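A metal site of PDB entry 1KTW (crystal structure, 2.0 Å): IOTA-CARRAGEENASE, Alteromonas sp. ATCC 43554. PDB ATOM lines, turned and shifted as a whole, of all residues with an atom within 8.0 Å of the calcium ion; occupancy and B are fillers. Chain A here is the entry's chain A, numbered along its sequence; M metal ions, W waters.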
ATOM      1  N   ASN A  62      16.437  23.434   4.773  1.00  0.00           N
ATOM      2  CA  ASN A  62      17.024  22.610   3.701  1.00  0.00           C
ATOM      3  C   ASN A  62      18.547  22.708   3.632  1.00  0.00           C
ATOM      4  O   ASN A  62      19.116  23.795   3.714  1.00  0.00           O
ATOM      5  CB  ASN A  62      16.409  22.971   2.337  1.00  0.00           C
ATOM      6  CG  ASN A  62      14.986  22.472   2.192  1.00  0.00           C
ATOM      7  OD1 ASN A  62      14.653  21.365   2.604  1.00  0.00           O
ATOM      8  ND2 ASN A  62      14.135  23.291   1.587  1.00  0.00           N
ATOM      9  N   GLU A  81      12.791  20.580   7.249  1.00  0.00           N
ATOM     10  CA  GLU A  81      12.292  20.828   5.881  1.00  0.00           C
ATOM     11  C   GLU A  81      12.435  19.609   4.951  1.00  0.00           C
ATOM     12  O   GLU A  81      13.295  18.751   5.159  1.00  0.00           O
ATOM     13  CB  GLU A  81      12.957  22.093   5.264  1.00  0.00           C
ATOM     14  CG  GLU A  81      12.571  23.425   6.008  1.00  0.00           C
ATOM     15  CD  GLU A  81      12.850  24.712   5.201  1.00  0.00           C
ATOM     16  OE1 GLU A  81      13.985  24.897   4.715  1.00  0.00           O
ATOM     17  OE2 GLU A  81      11.921  25.556   5.050  1.00  0.00           O
ATOM     18  N   SER A  82      11.577  19.565   3.940  1.00  0.00           N
ATOM     19  CA  SER A  82      11.488  18.432   3.000  1.00  0.00           C
ATOM     20  C   SER A  82      12.670  17.989   2.141  1.00  0.00           C
ATOM     21  O   SER A  82      12.663  16.861   1.634  1.00  0.00           O
ATOM     22  CB  SER A  82      10.285  18.637   2.083  1.00  0.00           C
ATOM     23  OG  SER A  82      10.019  17.440   1.381  1.00  0.00           O
ATOM     24  N   ASP A  83      13.665  18.840   1.947  1.00  0.00           N
ATOM     25  CA  ASP A  83      14.834  18.449   1.137  1.00  0.00           C
ATOM     26  C   ASP A  83      16.094  18.297   1.984  1.00  0.00           C
ATOM     27  O   ASP A  83      17.209  18.321   1.459  1.00  0.00           O
ATOM     28  CB  ASP A  83      15.102  19.478   0.029  1.00  0.00           C
ATOM     29  CG  ASP A  83      14.098  19.387  -1.104  1.00  0.00           C
ATOM     30  OD1 ASP A  83      13.729  18.262  -1.499  1.00  0.00           O
ATOM     31  OD2 ASP A  83      13.685  20.448  -1.619  1.00  0.00           O
ATOM     32  N   VAL A  84      15.923  18.149   3.290  1.00  0.00           N
ATOM     33  CA  VAL A  84      17.037  17.999   4.206  1.00  0.00           C
ATOM     34  C   VAL A  84      17.629  16.581   4.125  1.00  0.00           C
ATOM     35  O   VAL A  84      16.903  15.610   3.889  1.00  0.00           O
ATOM     36  CB  VAL A  84      16.578  18.273   5.676  1.00  0.00           C
ATOM     37  CG1 VAL A  84      17.572  17.711   6.661  1.00  0.00           C
ATOM     38  CG2 VAL A  84      16.425  19.778   5.899  1.00  0.00           C
ATOM     39  N   LEU A 116       8.612  17.830   7.669  1.00  0.00           N
ATOM     40  CA  LEU A 116       7.540  18.538   6.966  1.00  0.00           C
ATOM     41  C   LEU A 116       7.314  17.934   5.561  1.00  0.00           C
ATOM     42  O   LEU A 116       8.199  17.260   5.007  1.00  0.00           O
ATOM     43  CB  LEU A 116       7.921  20.028   6.827  1.00  0.00           C
ATOM     44  CG  LEU A 116       8.085  20.833   8.141  1.00  0.00           C
ATOM     45  CD1 LEU A 116       8.882  22.119   7.872  1.00  0.00           C
ATOM     46  CD2 LEU A 116       6.716  21.161   8.717  1.00  0.00           C
ATOM     47  N   GLY A 117       6.128  18.152   5.002  1.00  0.00           N
ATOM     48  CA  GLY A 117       5.847  17.684   3.644  1.00  0.00           C
ATOM     49  C   GLY A 117       5.982  16.192   3.431  1.00  0.00           C
ATOM     50  O   GLY A 117       5.464  15.394   4.216  1.00  0.00           O
ATOM     51  N   ASN A 118       6.693  15.799   2.369  1.00  0.00           N
ATOM     52  CA  ASN A 118       6.865  14.383   2.082  1.00  0.00           C
ATOM     53  C   ASN A 118       8.021  13.703   2.819  1.00  0.00           C
ATOM     54  O   ASN A 118       8.397  12.574   2.483  1.00  0.00           O
ATOM     55  CB  ASN A 118       6.952  14.112   0.560  1.00  0.00           C
ATOM     56  CG  ASN A 118       8.216  14.659  -0.097  1.00  0.00           C
ATOM     57  OD1 ASN A 118       9.193  15.023   0.572  1.00  0.00           O
ATOM     58  ND2 ASN A 118       8.208  14.693  -1.433  1.00  0.00           N
ATOM     59  N   GLY A 119       8.562  14.377   3.848  1.00  0.00           N
ATOM     60  CA  GLY A 119       9.637  13.815   4.657  1.00  0.00           C
ATOM     61  C   GLY A 119      11.058  14.105   4.200  1.00  0.00           C
ATOM     62  O   GLY A 119      11.267  14.527   3.070  1.00  0.00           O
ATOM     63  N   PHE A 120      12.033  13.876   5.084  1.00  0.00           N
ATOM     64  CA  PHE A 120      13.438  14.100   4.725  1.00  0.00           C
ATOM     65  C   PHE A 120      14.201  12.779   4.683  1.00  0.00           C
ATOM     66  O   PHE A 120      13.597  11.700   4.817  1.00  0.00           O
ATOM     67  CB  PHE A 120      14.122  15.077   5.714  1.00  0.00           C
ATOM     68  CG  PHE A 120      14.090  14.628   7.155  1.00  0.00           C
ATOM     69  CD1 PHE A 120      12.956  14.856   7.946  1.00  0.00           C
ATOM     70  CD2 PHE A 120      15.174  13.960   7.716  1.00  0.00           C
ATOM     71  CE1 PHE A 120      12.911  14.418   9.286  1.00  0.00           C
ATOM     72  CE2 PHE A 120      15.136  13.515   9.057  1.00  0.00           C
ATOM     73  CZ  PHE A 120      14.007  13.745   9.835  1.00  0.00           C
ATOM     74  N   LEU A 121      15.525  12.866   4.502  1.00  0.00           N
ATOM     75  CA  LEU A 121      16.381  11.676   4.415  1.00  0.00           C
ATOM     76  C   LEU A 121      17.490  11.573   5.457  1.00  0.00           C
ATOM     77  O   LEU A 121      18.162  12.559   5.744  1.00  0.00           O
ATOM     78  CB  LEU A 121      17.055  11.614   3.025  1.00  0.00           C
ATOM     79  CG  LEU A 121      17.980  10.411   2.748  1.00  0.00           C
ATOM     80  CD1 LEU A 121      17.123   9.146   2.534  1.00  0.00           C
ATOM     81  CD2 LEU A 121      18.850  10.691   1.488  1.00  0.00           C
ATOM     82  N   ASN A 147       7.892  11.056  10.128  1.00  0.00           N
ATOM     83  CA  ASN A 147       8.120  11.444   8.719  1.00  0.00           C
ATOM     84  C   ASN A 147       9.501  11.581   8.080  1.00  0.00           C
ATOM     85  O   ASN A 147       9.972  12.709   7.836  1.00  0.00           O
ATOM     86  CB  ASN A 147       7.317  12.743   8.469  1.00  0.00           C
ATOM     87  CG  ASN A 147       6.943  12.948   6.987  1.00  0.00           C
ATOM     88  OD1 ASN A 147       6.904  12.010   6.186  1.00  0.00           O
ATOM     89  ND2 ASN A 147       6.628  14.198   6.635  1.00  0.00           N
ATOM     90  N   PHE A 148      10.109  10.446   7.743  1.00  0.00           N
ATOM     91  CA  PHE A 148      11.404  10.428   7.057  1.00  0.00           C
ATOM     92  C   PHE A 148      11.746   9.057   6.474  1.00  0.00           C
ATOM     93  O   PHE A 148      11.075   8.057   6.771  1.00  0.00           O
ATOM     94  CB  PHE A 148      12.555  10.951   7.951  1.00  0.00           C
ATOM     95  CG  PHE A 148      12.679  10.277   9.323  1.00  0.00           C
ATOM     96  CD1 PHE A 148      13.550   9.197   9.532  1.00  0.00           C
ATOM     97  CD2 PHE A 148      11.923  10.743  10.410  1.00  0.00           C
ATOM     98  CE1 PHE A 148      13.677   8.603  10.804  1.00  0.00           C
ATOM     99  CE2 PHE A 148      12.053  10.166  11.686  1.00  0.00           C
ATOM    100  CZ  PHE A 148      12.922   9.095  11.879  1.00  0.00           C
ATOM    101  N   THR A 149      12.768   9.031   5.627  1.00  0.00           N
ATOM    102  CA  THR A 149      13.272   7.804   5.010  1.00  0.00           C
ATOM    103  C   THR A 149      14.693   7.585   5.511  1.00  0.00           C
ATOM    104  O   THR A 149      15.430   8.545   5.703  1.00  0.00           O
ATOM    105  CB  THR A 149      13.296   7.937   3.458  1.00  0.00           C
ATOM    106  OG1 THR A 149      11.966   8.104   2.968  1.00  0.00           O
ATOM    107  CG2 THR A 149      13.921   6.678   2.813  1.00  0.00           C
HETATM  108 CA    CA M   1      11.460  14.993   0.702  1.00  0.00          CA
HETATM  109  O   HOH W   1      10.655  12.443   0.778  1.00  0.00           O
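Within 4 Å of the calcium ion: Ser 82, Asn 118 and Gly 119. Along chain A the residues within 4 Å of the calcium ion span positions 82 to 119. The nearest printed residue that does not touch the calcium ion is Asp 83 (4.5 Å).
The calcium ion is bound by the side-chain amide oxygen (OD1) of Asn 118, the backbone carbonyl oxygen (O) of Ser 82, the backbone carbonyl oxygen (O) of Gly 119 and water W1. Slightly farther from the calcium ion lies the side-chain hydroxyl (OG) of Ser 82 (2.9 Å).
N of Gly 119 sits close to ND2 of Asn 147 (3.4 Å).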
